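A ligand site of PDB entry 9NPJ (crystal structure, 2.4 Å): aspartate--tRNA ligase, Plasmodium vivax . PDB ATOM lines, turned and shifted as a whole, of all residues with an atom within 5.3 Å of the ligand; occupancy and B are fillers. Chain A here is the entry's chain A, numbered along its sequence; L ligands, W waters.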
ATOM      1  N   GLN A 276      29.460 -25.874 -21.547  1.00  0.00           N
ATOM      2  CA  GLN A 276      28.579 -24.997 -20.807  1.00  0.00           C
ATOM      3  C   GLN A 276      27.692 -25.760 -19.830  1.00  0.00           C
ATOM      4  O   GLN A 276      27.076 -25.150 -18.953  1.00  0.00           O
ATOM      5  CB  GLN A 276      27.708 -24.199 -21.780  1.00  0.00           C
ATOM      6  CG  GLN A 276      28.534 -23.214 -22.600  1.00  0.00           C
ATOM      7  CD  GLN A 276      27.764 -22.723 -23.803  1.00  0.00           C
ATOM      8  OE1 GLN A 276      27.787 -23.336 -24.859  1.00  0.00           O
ATOM      9  NE2 GLN A 276      27.045 -21.619 -23.635  1.00  0.00           N
ATOM     10  N   SER A 277      27.641 -27.078 -19.963  1.00  0.00           N
ATOM     11  CA  SER A 277      26.737 -27.912 -19.209  1.00  0.00           C
ATOM     12  C   SER A 277      27.010 -29.366 -19.573  1.00  0.00           C
ATOM     13  O   SER A 277      27.468 -29.644 -20.682  1.00  0.00           O
ATOM     14  CB  SER A 277      25.290 -27.539 -19.536  1.00  0.00           C
ATOM     15  OG  SER A 277      24.482 -28.688 -19.544  1.00  0.00           O
ATOM     16  N   GLN A 279      24.730 -31.454 -20.162  1.00  0.00           N
ATOM     17  CA  GLN A 279      23.467 -31.842 -20.793  1.00  0.00           C
ATOM     18  C   GLN A 279      23.593 -33.086 -21.677  1.00  0.00           C
ATOM     19  O   GLN A 279      22.964 -34.118 -21.408  1.00  0.00           O
ATOM     20  CB  GLN A 279      22.923 -30.672 -21.617  1.00  0.00           C
ATOM     21  CG  GLN A 279      21.604 -30.971 -22.264  1.00  0.00           C
ATOM     22  CD  GLN A 279      20.529 -31.167 -21.234  1.00  0.00           C
ATOM     23  OE1 GLN A 279      20.519 -30.515 -20.188  1.00  0.00           O
ATOM     24  NE2 GLN A 279      19.612 -32.088 -21.520  1.00  0.00           N
ATOM     25  N   LYS A 282      24.900 -36.397 -19.790  1.00  0.00           N
ATOM     26  CA  LYS A 282      24.015 -37.024 -18.809  1.00  0.00           C
ATOM     27  C   LYS A 282      22.858 -37.733 -19.516  1.00  0.00           C
ATOM     28  O   LYS A 282      22.453 -38.829 -19.108  1.00  0.00           O
ATOM     29  CB  LYS A 282      23.508 -36.007 -17.771  1.00  0.00           C
ATOM     30  CG  LYS A 282      22.656 -34.857 -18.282  1.00  0.00           C
ATOM     31  CD  LYS A 282      22.228 -33.949 -17.122  1.00  0.00           C
ATOM     32  CE  LYS A 282      21.448 -32.736 -17.604  1.00  0.00           C
ATOM     33  NZ  LYS A 282      20.939 -31.873 -16.499  1.00  0.00           N
ATOM     34  N   ARG A 301      30.948 -20.557 -18.988  1.00  0.00           N
ATOM     35  CA  ARG A 301      30.018 -19.788 -19.812  1.00  0.00           C
ATOM     36  C   ARG A 301      30.597 -18.413 -20.113  1.00  0.00           C
ATOM     37  O   ARG A 301      30.843 -17.624 -19.195  1.00  0.00           O
ATOM     38  CB  ARG A 301      28.666 -19.689 -19.121  1.00  0.00           C
ATOM     39  CG  ARG A 301      27.984 -21.031 -19.133  1.00  0.00           C
ATOM     40  CD  ARG A 301      26.609 -21.025 -18.561  1.00  0.00           C
ATOM     41  NE  ARG A 301      26.094 -22.393 -18.601  1.00  0.00           N
ATOM     42  CZ  ARG A 301      24.824 -22.718 -18.482  1.00  0.00           C
ATOM     43  NH1 ARG A 301      23.872 -21.806 -18.334  1.00  0.00           N
ATOM     44  NH2 ARG A 301      24.492 -24.007 -18.512  1.00  0.00           N
ATOM     45  N   GLU A 303      29.594 -15.481 -21.124  1.00  0.00           N
ATOM     46  CA  GLU A 303      28.640 -14.377 -21.204  1.00  0.00           C
ATOM     47  C   GLU A 303      29.411 -13.100 -20.922  1.00  0.00           C
ATOM     48  O   GLU A 303      29.843 -12.888 -19.786  1.00  0.00           O
ATOM     49  CB  GLU A 303      27.492 -14.548 -20.214  1.00  0.00           C
ATOM     50  CG  GLU A 303      27.241 -15.987 -19.741  1.00  0.00           C
ATOM     51  CD  GLU A 303      26.048 -16.090 -18.762  1.00  0.00           C
ATOM     52  OE1 GLU A 303      25.476 -17.214 -18.644  1.00  0.00           O
ATOM     53  OE2 GLU A 303      25.686 -15.068 -18.129  1.00  0.00           O
ATOM     54  N   ARG A 309      24.803 -11.395 -10.654  1.00  0.00           N
ATOM     55  CA  ARG A 309      24.125 -12.669 -10.440  1.00  0.00           C
ATOM     56  C   ARG A 309      24.660 -13.846 -11.243  1.00  0.00           C
ATOM     57  O   ARG A 309      24.281 -14.985 -10.962  1.00  0.00           O
ATOM     58  CB  ARG A 309      22.626 -12.500 -10.692  1.00  0.00           C
ATOM     59  CG  ARG A 309      22.012 -11.384  -9.833  1.00  0.00           C
ATOM     60  CD  ARG A 309      21.418 -11.934  -8.538  1.00  0.00           C
ATOM     61  NE  ARG A 309      21.754 -11.137  -7.352  1.00  0.00           N
ATOM     62  CZ  ARG A 309      21.277 -11.382  -6.129  1.00  0.00           C
ATOM     63  NH1 ARG A 309      20.358 -12.304  -5.913  1.00  0.00           N
ATOM     64  NH2 ARG A 309      21.761 -10.682  -5.090  1.00  0.00           N
ATOM     65  N   HIS A 310      25.561 -13.615 -12.210  1.00  0.00           N
ATOM     66  CA  HIS A 310      26.114 -14.695 -13.028  1.00  0.00           C
ATOM     67  C   HIS A 310      27.636 -14.617 -13.015  1.00  0.00           C
ATOM     68  O   HIS A 310      28.229 -13.571 -12.730  1.00  0.00           O
ATOM     69  CB  HIS A 310      25.599 -14.639 -14.486  1.00  0.00           C
ATOM     70  CG  HIS A 310      24.299 -15.359 -14.694  1.00  0.00           C
ATOM     71  ND1 HIS A 310      23.810 -15.652 -15.958  1.00  0.00           N
ATOM     72  CD2 HIS A 310      23.388 -15.852 -13.816  1.00  0.00           C
ATOM     73  CE1 HIS A 310      22.662 -16.316 -15.837  1.00  0.00           C
ATOM     74  NE2 HIS A 310      22.381 -16.437 -14.551  1.00  0.00           N
ATOM     75  N   LEU A 311      28.271 -15.747 -13.319  1.00  0.00           N
ATOM     76  CA  LEU A 311      29.720 -15.823 -13.397  1.00  0.00           C
ATOM     77  C   LEU A 311      30.111 -16.553 -14.674  1.00  0.00           C
ATOM     78  O   LEU A 311      29.278 -17.196 -15.317  1.00  0.00           O
ATOM     79  CB  LEU A 311      30.296 -16.530 -12.165  1.00  0.00           C
ATOM     80  CG  LEU A 311      30.112 -15.797 -10.831  1.00  0.00           C
ATOM     81  CD1 LEU A 311      30.551 -16.657  -9.650  1.00  0.00           C
ATOM     82  CD2 LEU A 311      30.880 -14.474 -10.866  1.00  0.00           C
ATOM     83  N   CYS A 312      31.384 -16.441 -15.058  1.00  0.00           N
ATOM     84  CA  CYS A 312      31.822 -17.149 -16.251  1.00  0.00           C
ATOM     85  C   CYS A 312      32.213 -18.591 -15.958  1.00  0.00           C
ATOM     86  O   CYS A 312      32.426 -19.370 -16.898  1.00  0.00           O
ATOM     87  CB  CYS A 312      32.998 -16.392 -16.892  1.00  0.00           C
ATOM     88  SG  CYS A 312      32.531 -14.736 -17.485  1.00  0.00           S
ATOM     89  N   TYR A 314      31.061 -21.638 -12.875  1.00  0.00           N
ATOM     90  CA  TYR A 314      30.334 -21.935 -11.651  1.00  0.00           C
ATOM     91  C   TYR A 314      30.154 -23.435 -11.539  1.00  0.00           C
ATOM     92  O   TYR A 314      30.332 -24.179 -12.507  1.00  0.00           O
ATOM     93  CB  TYR A 314      28.987 -21.188 -11.589  1.00  0.00           C
ATOM     94  CG  TYR A 314      27.909 -21.740 -12.519  1.00  0.00           C
ATOM     95  CD1 TYR A 314      27.741 -21.240 -13.816  1.00  0.00           C
ATOM     96  CD2 TYR A 314      27.052 -22.750 -12.090  1.00  0.00           C
ATOM     97  CE1 TYR A 314      26.750 -21.736 -14.660  1.00  0.00           C
ATOM     98  CE2 TYR A 314      26.059 -23.242 -12.912  1.00  0.00           C
ATOM     99  CZ  TYR A 314      25.894 -22.743 -14.199  1.00  0.00           C
ATOM    100  OH  TYR A 314      24.893 -23.266 -15.012  1.00  0.00           O
ATOM    101  N   ASP A 318      23.682 -31.283 -11.518  1.00  0.00           N
ATOM    102  CA  ASP A 318      22.915 -31.807 -12.626  1.00  0.00           C
ATOM    103  C   ASP A 318      22.285 -33.137 -12.233  1.00  0.00           C
ATOM    104  O   ASP A 318      22.925 -33.984 -11.608  1.00  0.00           O
ATOM    105  CB  ASP A 318      23.797 -31.948 -13.869  1.00  0.00           C
ATOM    106  CG  ASP A 318      23.930 -30.638 -14.647  1.00  0.00           C
ATOM    107  OD1 ASP A 318      23.015 -30.339 -15.445  1.00  0.00           O
ATOM    108  OD2 ASP A 318      24.942 -29.910 -14.483  1.00  0.00           O
ATOM    109  N   VAL A 319      21.013 -33.292 -12.585  1.00  0.00           N
ATOM    110  CA  VAL A 319      20.259 -34.510 -12.375  1.00  0.00           C
ATOM    111  C   VAL A 319      19.635 -34.948 -13.701  1.00  0.00           C
ATOM    112  O   VAL A 319      19.146 -34.112 -14.463  1.00  0.00           O
ATOM    113  CB  VAL A 319      19.148 -34.329 -11.303  1.00  0.00           C
ATOM    114  CG1 VAL A 319      18.691 -35.689 -10.806  1.00  0.00           C
ATOM    115  CG2 VAL A 319      19.638 -33.473 -10.144  1.00  0.00           C
ATOM    116  N   GLU A 320      19.654 -36.254 -13.957  1.00  0.00           N
ATOM    117  CA  GLU A 320      18.961 -36.835 -15.102  1.00  0.00           C
ATOM    118  C   GLU A 320      18.415 -38.187 -14.683  1.00  0.00           C
ATOM    119  O   GLU A 320      19.124 -38.971 -14.039  1.00  0.00           O
ATOM    120  CB  GLU A 320      19.892 -36.960 -16.315  1.00  0.00           C
ATOM    121  CG  GLU A 320      19.173 -37.031 -17.668  1.00  0.00           C
ATOM    122  CD  GLU A 320      18.615 -35.670 -18.144  1.00  0.00           C
ATOM    123  OE1 GLU A 320      19.078 -34.596 -17.662  1.00  0.00           O
ATOM    124  OE2 GLU A 320      17.711 -35.684 -19.010  1.00  0.00           O
ATOM    125  N   TYR A 437      16.317 -29.792 -26.860  1.00  0.00           N
ATOM    126  CA  TYR A 437      16.053 -31.115 -26.307  1.00  0.00           C
ATOM    127  C   TYR A 437      14.766 -31.176 -25.496  1.00  0.00           C
ATOM    128  O   TYR A 437      14.414 -32.254 -25.017  1.00  0.00           O
ATOM    129  CB  TYR A 437      17.234 -31.592 -25.448  1.00  0.00           C
ATOM    130  CG  TYR A 437      17.761 -30.534 -24.505  1.00  0.00           C
ATOM    131  CD1 TYR A 437      17.094 -30.220 -23.324  1.00  0.00           C
ATOM    132  CD2 TYR A 437      18.930 -29.828 -24.805  1.00  0.00           C
ATOM    133  CE1 TYR A 437      17.580 -29.241 -22.473  1.00  0.00           C
ATOM    134  CE2 TYR A 437      19.418 -28.850 -23.944  1.00  0.00           C
ATOM    135  CZ  TYR A 437      18.733 -28.562 -22.792  1.00  0.00           C
ATOM    136  OH  TYR A 437      19.210 -27.590 -21.950  1.00  0.00           O
ATOM    137  N   GLU A 459      15.806 -17.448 -10.470  1.00  0.00           N
ATOM    138  CA  GLU A 459      15.826 -18.815 -10.952  1.00  0.00           C
ATOM    139  C   GLU A 459      17.016 -19.570 -10.345  1.00  0.00           C
ATOM    140  O   GLU A 459      18.150 -19.087 -10.378  1.00  0.00           O
ATOM    141  CB  GLU A 459      15.908 -18.805 -12.477  1.00  0.00           C
ATOM    142  CG  GLU A 459      16.452 -20.069 -13.073  1.00  0.00           C
ATOM    143  CD  GLU A 459      16.637 -19.985 -14.577  1.00  0.00           C
ATOM    144  OE1 GLU A 459      16.143 -19.009 -15.218  1.00  0.00           O
ATOM    145  OE2 GLU A 459      17.288 -20.912 -15.123  1.00  0.00           O
ATOM    146  N   ILE A 460      16.742 -20.743  -9.742  1.00  0.00           N
ATOM    147  CA  ILE A 460      17.798 -21.608  -9.235  1.00  0.00           C
ATOM    148  C   ILE A 460      17.937 -22.893 -10.033  1.00  0.00           C
ATOM    149  O   ILE A 460      19.018 -23.498 -10.006  1.00  0.00           O
ATOM    150  CB  ILE A 460      17.605 -21.950  -7.747  1.00  0.00           C
ATOM    151  CG1 ILE A 460      16.155 -22.378  -7.474  1.00  0.00           C
ATOM    152  CG2 ILE A 460      18.093 -20.819  -6.848  1.00  0.00           C
ATOM    153  CD1 ILE A 460      16.040 -23.630  -6.590  1.00  0.00           C
ATOM    154  N   LEU A 461      16.870 -23.353 -10.695  1.00  0.00           N
ATOM    155  CA  LEU A 461      16.855 -24.637 -11.377  1.00  0.00           C
ATOM    156  C   LEU A 461      16.104 -24.481 -12.685  1.00  0.00           C
ATOM    157  O   LEU A 461      15.166 -23.689 -12.784  1.00  0.00           O
ATOM    158  CB  LEU A 461      16.228 -25.739 -10.521  1.00  0.00           C
ATOM    159  CG  LEU A 461      15.848 -27.109 -11.122  1.00  0.00           C
ATOM    160  CD1 LEU A 461      15.619 -28.143 -10.004  1.00  0.00           C
ATOM    161  CD2 LEU A 461      14.605 -27.025 -12.008  1.00  0.00           C
ATOM    162  N   SER A 462      16.541 -25.231 -13.685  1.00  0.00           N
ATOM    163  CA  SER A 462      15.896 -25.278 -14.993  1.00  0.00           C
ATOM    164  C   SER A 462      16.009 -26.705 -15.528  1.00  0.00           C
ATOM    165  O   SER A 462      17.063 -27.332 -15.422  1.00  0.00           O
ATOM    166  CB  SER A 462      16.541 -24.260 -15.946  1.00  0.00           C
ATOM    167  OG  SER A 462      15.837 -24.168 -17.170  1.00  0.00           O
ATOM    168  N   GLY A 463      14.914 -27.231 -16.054  1.00  0.00           N
ATOM    169  CA  GLY A 463      14.967 -28.598 -16.556  1.00  0.00           C
ATOM    170  C   GLY A 463      13.795 -28.868 -17.470  1.00  0.00           C
ATOM    171  O   GLY A 463      12.991 -27.982 -17.763  1.00  0.00           O
ATOM    172  N   SER A 464      13.696 -30.119 -17.916  1.00  0.00           N
ATOM    173  CA  SER A 464      12.522 -30.476 -18.725  1.00  0.00           C
ATOM    174  C   SER A 464      12.452 -31.977 -18.957  1.00  0.00           C
ATOM    175  O   SER A 464      13.468 -32.688 -18.849  1.00  0.00           O
ATOM    176  CB  SER A 464      12.552 -29.779 -20.076  1.00  0.00           C
ATOM    177  OG  SER A 464      13.463 -30.441 -20.936  1.00  0.00           O
ATOM    178  N   ARG A 466      12.574 -34.741 -21.617  1.00  0.00           N
ATOM    179  CA  ARG A 466      13.412 -34.746 -22.802  1.00  0.00           C
ATOM    180  C   ARG A 466      12.690 -35.383 -23.977  1.00  0.00           C
ATOM    181  O   ARG A 466      11.801 -36.221 -23.822  1.00  0.00           O
ATOM    182  CB  ARG A 466      14.734 -35.496 -22.565  1.00  0.00           C
ATOM    183  CG  ARG A 466      15.527 -35.114 -21.303  1.00  0.00           C
ATOM    184  CD  ARG A 466      15.814 -33.603 -21.110  1.00  0.00           C
ATOM    185  NE  ARG A 466      16.723 -33.431 -19.987  1.00  0.00           N
ATOM    186  CZ  ARG A 466      16.969 -32.284 -19.353  1.00  0.00           C
ATOM    187  NH1 ARG A 466      16.361 -31.159 -19.684  1.00  0.00           N
ATOM    188  NH2 ARG A 466      17.856 -32.270 -18.356  1.00  0.00           N
ATOM    189  N   GLY A 503      15.421 -34.117 -16.641  1.00  0.00           N
ATOM    190  CA  GLY A 503      16.585 -33.695 -15.885  1.00  0.00           C
ATOM    191  C   GLY A 503      16.466 -32.239 -15.501  1.00  0.00           C
ATOM    192  O   GLY A 503      15.492 -31.555 -15.832  1.00  0.00           O
ATOM    193  N   CYS A 504      17.486 -31.765 -14.782  1.00  0.00           N
ATOM    194  CA  CYS A 504      17.529 -30.365 -14.377  1.00  0.00           C
ATOM    195  C   CYS A 504      18.966 -29.976 -14.098  1.00  0.00           C
ATOM    196  O   CYS A 504      19.831 -30.826 -13.859  1.00  0.00           O
ATOM    197  CB  CYS A 504      16.649 -30.113 -13.143  1.00  0.00           C
ATOM    198  SG  CYS A 504      17.052 -31.172 -11.713  1.00  0.00           S
ATOM    199  N   GLY A 505      19.226 -28.681 -14.172  1.00  0.00           N
ATOM    200  CA  GLY A 505      20.525 -28.144 -13.795  1.00  0.00           C
ATOM    201  C   GLY A 505      20.349 -27.014 -12.806  1.00  0.00           C
ATOM    202  O   GLY A 505      19.431 -26.212 -12.909  1.00  0.00           O
ATOM    203  N   ILE A 506      21.279 -26.947 -11.836  1.00  0.00           N
ATOM    204  CA  ILE A 506      21.170 -26.087 -10.675  1.00  0.00           C
ATOM    205  C   ILE A 506      22.489 -25.354 -10.439  1.00  0.00           C
ATOM    206  O   ILE A 506      23.562 -25.951 -10.523  1.00  0.00           O
ATOM    207  CB  ILE A 506      20.816 -26.917  -9.427  1.00  0.00           C
ATOM    208  CG1 ILE A 506      19.498 -27.674  -9.645  1.00  0.00           C
ATOM    209  CG2 ILE A 506      20.866 -26.039  -8.152  1.00  0.00           C
ATOM    210  CD1 ILE A 506      19.339 -28.905  -8.746  1.00  0.00           C
ATOM    211  N   GLY A 507      22.395 -24.049 -10.132  1.00  0.00           N
ATOM    212  CA  GLY A 507      23.559 -23.287  -9.735  1.00  0.00           C
ATOM    213  C   GLY A 507      23.816 -23.373  -8.239  1.00  0.00           C
ATOM    214  O   GLY A 507      23.009 -22.879  -7.426  1.00  0.00           O
ATOM    215  N   GLU A 509      26.248 -21.934  -6.334  1.00  0.00           N
ATOM    216  CA  GLU A 509      26.481 -20.621  -5.762  1.00  0.00           C
ATOM    217  C   GLU A 509      25.195 -19.808  -5.709  1.00  0.00           C
ATOM    218  O   GLU A 509      24.957 -19.071  -4.746  1.00  0.00           O
ATOM    219  CB  GLU A 509      27.568 -19.878  -6.578  1.00  0.00           C
ATOM    220  CG  GLU A 509      28.897 -20.644  -6.720  1.00  0.00           C
ATOM    221  CD  GLU A 509      28.918 -21.617  -7.921  1.00  0.00           C
ATOM    222  OE1 GLU A 509      27.838 -22.086  -8.382  1.00  0.00           O
ATOM    223  OE2 GLU A 509      30.035 -21.935  -8.404  1.00  0.00           O
ATOM    224  N   ARG A 510      24.347 -19.915  -6.727  1.00  0.00           N
ATOM    225  CA  ARG A 510      23.100 -19.161  -6.734  1.00  0.00           C
ATOM    226  C   ARG A 510      22.139 -19.647  -5.643  1.00  0.00           C
ATOM    227  O   ARG A 510      21.460 -18.829  -5.017  1.00  0.00           O
ATOM    228  CB  ARG A 510      22.442 -19.241  -8.115  1.00  0.00           C
ATOM    229  CG  ARG A 510      23.098 -18.313  -9.134  1.00  0.00           C
ATOM    230  CD  ARG A 510      22.471 -18.455 -10.520  1.00  0.00           C
ATOM    231  NE  ARG A 510      21.049 -18.132 -10.526  1.00  0.00           N
ATOM    232  CZ  ARG A 510      20.571 -16.899 -10.548  1.00  0.00           C
ATOM    233  NH1 ARG A 510      21.383 -15.849 -10.500  1.00  0.00           N
ATOM    234  NH2 ARG A 510      19.255 -16.711 -10.629  1.00  0.00           N
ATOM    235  N   ILE A 521      26.592 -12.657  -6.366  1.00  0.00           N
ATOM    236  CA  ILE A 521      27.042 -14.040  -6.572  1.00  0.00           C
ATOM    237  C   ILE A 521      28.515 -14.203  -6.187  1.00  0.00           C
ATOM    238  O   ILE A 521      28.951 -15.298  -5.815  1.00  0.00           O
ATOM    239  CB  ILE A 521      26.794 -14.455  -8.032  1.00  0.00           C
ATOM    240  CG1 ILE A 521      27.229 -15.905  -8.284  1.00  0.00           C
ATOM    241  CG2 ILE A 521      27.539 -13.537  -9.004  1.00  0.00           C
ATOM    242  CD1 ILE A 521      26.329 -16.894  -7.695  1.00  0.00           C
HETATM  243  C1  LIG L   1      21.221 -23.113 -13.741  1.00  0.00           C
HETATM  244  C2  LIG L   1      22.614 -21.538 -13.097  1.00  0.00           C
HETATM  245  C3  LIG L   1      24.358 -19.875 -13.691  1.00  0.00           C
HETATM  246  C4  LIG L   1      24.788 -19.279 -14.851  1.00  0.00           C
HETATM  247  C5  LIG L   1      18.626 -28.939 -17.792  1.00  0.00           C
HETATM  248  C6  LIG L   1      19.516 -27.764 -17.397  1.00  0.00           C
HETATM  249  C7  LIG L   1      20.174 -27.037 -18.565  1.00  0.00           C
HETATM  250  C8  LIG L   1      20.871 -25.845 -17.906  1.00  0.00           C
HETATM  251  C9  LIG L   1      21.022 -24.067 -14.867  1.00  0.00           C
HETATM  252  C10 LIG L   1      23.174 -20.615 -15.343  1.00  0.00           C
HETATM  253  C11 LIG L   1      25.922 -18.722 -12.484  1.00  0.00           C
HETATM  254  C12 LIG L   1      25.855 -18.375 -14.765  1.00  0.00           C
HETATM  255  C13 LIG L   1      20.431 -22.007 -13.846  1.00  0.00           C
HETATM  256  C14 LIG L   1      21.134 -21.039 -12.879  1.00  0.00           C
HETATM  257  N1  LIG L   1      21.158 -27.850 -19.264  1.00  0.00           N
HETATM  258  N2  LIG L   1      19.950 -24.742 -18.006  1.00  0.00           N
HETATM  259  N3  LIG L   1      23.344 -20.692 -14.031  1.00  0.00           N
HETATM  260  N4  LIG L   1      24.041 -19.757 -15.855  1.00  0.00           N
HETATM  261  N5  LIG L   1      24.938 -19.594 -12.516  1.00  0.00           N
HETATM  262  N6  LIG L   1      26.383 -18.130 -13.580  1.00  0.00           N
HETATM  263  N7  LIG L   1      26.391 -17.707 -15.926  1.00  0.00           N
HETATM  264  O1  LIG L   1      18.833 -30.046 -17.232  1.00  0.00           O
HETATM  265  O2  LIG L   1      17.700 -28.762 -18.652  1.00  0.00           O
HETATM  266  O3  LIG L   1      22.096 -25.546 -18.527  1.00  0.00           O
HETATM  267  O4  LIG L   1      19.231 -22.399 -16.959  1.00  0.00           O
HETATM  268  O5  LIG L   1      21.128 -22.475 -18.436  1.00  0.00           O
HETATM  269  O6  LIG L   1      21.460 -23.456 -16.070  1.00  0.00           O
HETATM  270  O7  LIG L   1      22.500 -22.766 -13.558  1.00  0.00           O
HETATM  271  O8  LIG L   1      19.039 -22.234 -13.368  1.00  0.00           O
HETATM  272  O9  LIG L   1      20.822 -21.340 -11.625  1.00  0.00           O
HETATM  273  S1  LIG L   1      20.426 -23.252 -17.356  1.00  0.00           S
HETATM  274 CL1  LIG L   1      26.675 -18.332 -10.917  1.00  0.00          CL
HETATM  275  O   HOH W   1      23.140 -28.173 -16.857  1.00  0.00           O
HETATM  276  O   HOH W   2      16.340 -26.801 -19.818  1.00  0.00           O
HETATM  277  O   HOH W   3      17.232 -24.316 -19.372  1.00  0.00           O
HETATM  278  O   HOH W   4      19.904 -19.427 -16.481  1.00  0.00           O
HETATM  279  O   HOH W   5      25.481 -20.699  -9.272  1.00  0.00           O
HETATM  280  O   HOH W   6      17.034 -21.136 -18.586  1.00  0.00           O
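N of Leu 461 touches O8 of the ligand, 3.6 Å away.
Ser 462 touches the ligand.
Gly 463 touches the ligand (CA to O2, 3.4 Å).
Gly 503 touches the ligand (C to O1, 3.7 Å).
Ile 521 touches the ligand (CD1 to CL1, 3.5 Å).
Within 4 Å of the ligand: Ser 277, Gln 279, Lys 282, Arg 301, Glu 303, His 310, Leu 311, Tyr 314, Tyr 437, Glu 459, Ile 460, Leu 461, Ser 462, Gly 463, Arg 466, Gly 503, Cys 504, Gly 505, Gly 507, Arg 510 and Ile 521.
NH2 of Arg 466 lies within salt-bridge range of O1 of the ligand (2.7 Å).
The side-chain carboxylate (OE2) of Glu 459 sits at hydrogen-bond distance from an oxygen (O8) of the ligand (2.8 Å).
NH1 of Arg 301 is in hydrogen-bond range of O5 of the ligand (2.8 Å).
The side-chain hydroxyl (OH) of Tyr 314 lies within hydrogen-bond range of an oxygen (O7) of the ligand.
The side-chain amino group (NZ) of Lys 282 is in salt-bridge range of an oxygen (O1) of the ligand (2.9 Å).
OE1 of Gln 279 is in hydrogen-bond range of N1 of the ligand, at 2.9 Å.
N7 of the ligand is in hydrogen-bond range of OE1 of Glu 303 (2.9 Å).
A nitrogen (N6) of the ligand sits at hydrogen-bond distance from the backbone NH (N) of Leu 311 (3.1 Å).
The backbone carbonyl oxygen (O) of Leu 311 is in hydrogen-bond range of a nitrogen (N7) of the ligand (3.0 Å).
The backbone NH (N) of Cys 504 lies close to an oxygen (O1) of the ligand (3.3 Å).
The backbone carbonyl oxygen of Ile 460 sits at hydrogen-bond distance from an oxygen (O9) of the ligand (3.2 Å).
ND1 of His 310 lies within hydrogen-bond range of N7 of the ligand.
The backbone NH of Gly 505 sits close to an oxygen (O1) of the ligand, 3.4 Å away.
OH of Tyr 437 lies within hydrogen-bond range of N1 of the ligand (3.3 Å).
NE of Arg 510 is in hydrogen-bond range of O9 of the ligand (3.4 Å).
OG of Ser 277 sits at hydrogen-bond distance from N1 of the ligand, 3.4 Å away.
The backbone NH of Gly 507 lies within hydrogen-bond range of an oxygen (O9) of the ligand (3.5 Å).
Water W6 bridges an oxygen (O4) of the ligand and the side-chain carboxylate (OE2) of Glu 459.
Water W3 lies within hydrogen-bond range of OG of Ser 462 and N2 of the ligand.
Water W4 bridges an oxygen (O4) of the ligand (3.1 Å) and the side-chain carboxylate of Glu 459 (3.3 Å).
Water W5 lies within hydrogen-bond range of the side-chain carboxylate of Glu 509, the backbone NH of Arg 510 and a nitrogen (N5) of the ligand.
Water W1 lies within hydrogen-bond range of OD1 of Asp 318 (2.6 Å), OG of Ser 277 (3.0 Å) and N1 of the ligand (3.1 Å).
The guanidinium group (NH1) of Arg 466 is in hydrogen-bond range of the side-chain hydroxyl (OG) of Ser 464, at 3.2 Å.
OE2 of Glu 320 is in salt-bridge range of NE of Arg 466, 2.6 Å away.
NH2 of Arg 301 is in hydrogen-bond range of O of Gln 276 (2.9 Å).
The backbone carbonyl oxygen (O) of Cys 312 sits at hydrogen-bond distance from the backbone NH (N) of Arg 301.
OE2 of Glu 303 lies within hydrogen-bond range of ND1 of His 310 (2.9 Å).
O of Ser 462 lies within hydrogen-bond range of N of Gly 505 (2.8 Å).
O of Ile 460 is in hydrogen-bond range of N of Gly 507 (3.4 Å).
N of Ser 464 lies within hydrogen-bond range of O of Gly 503, at 3.1 Å.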
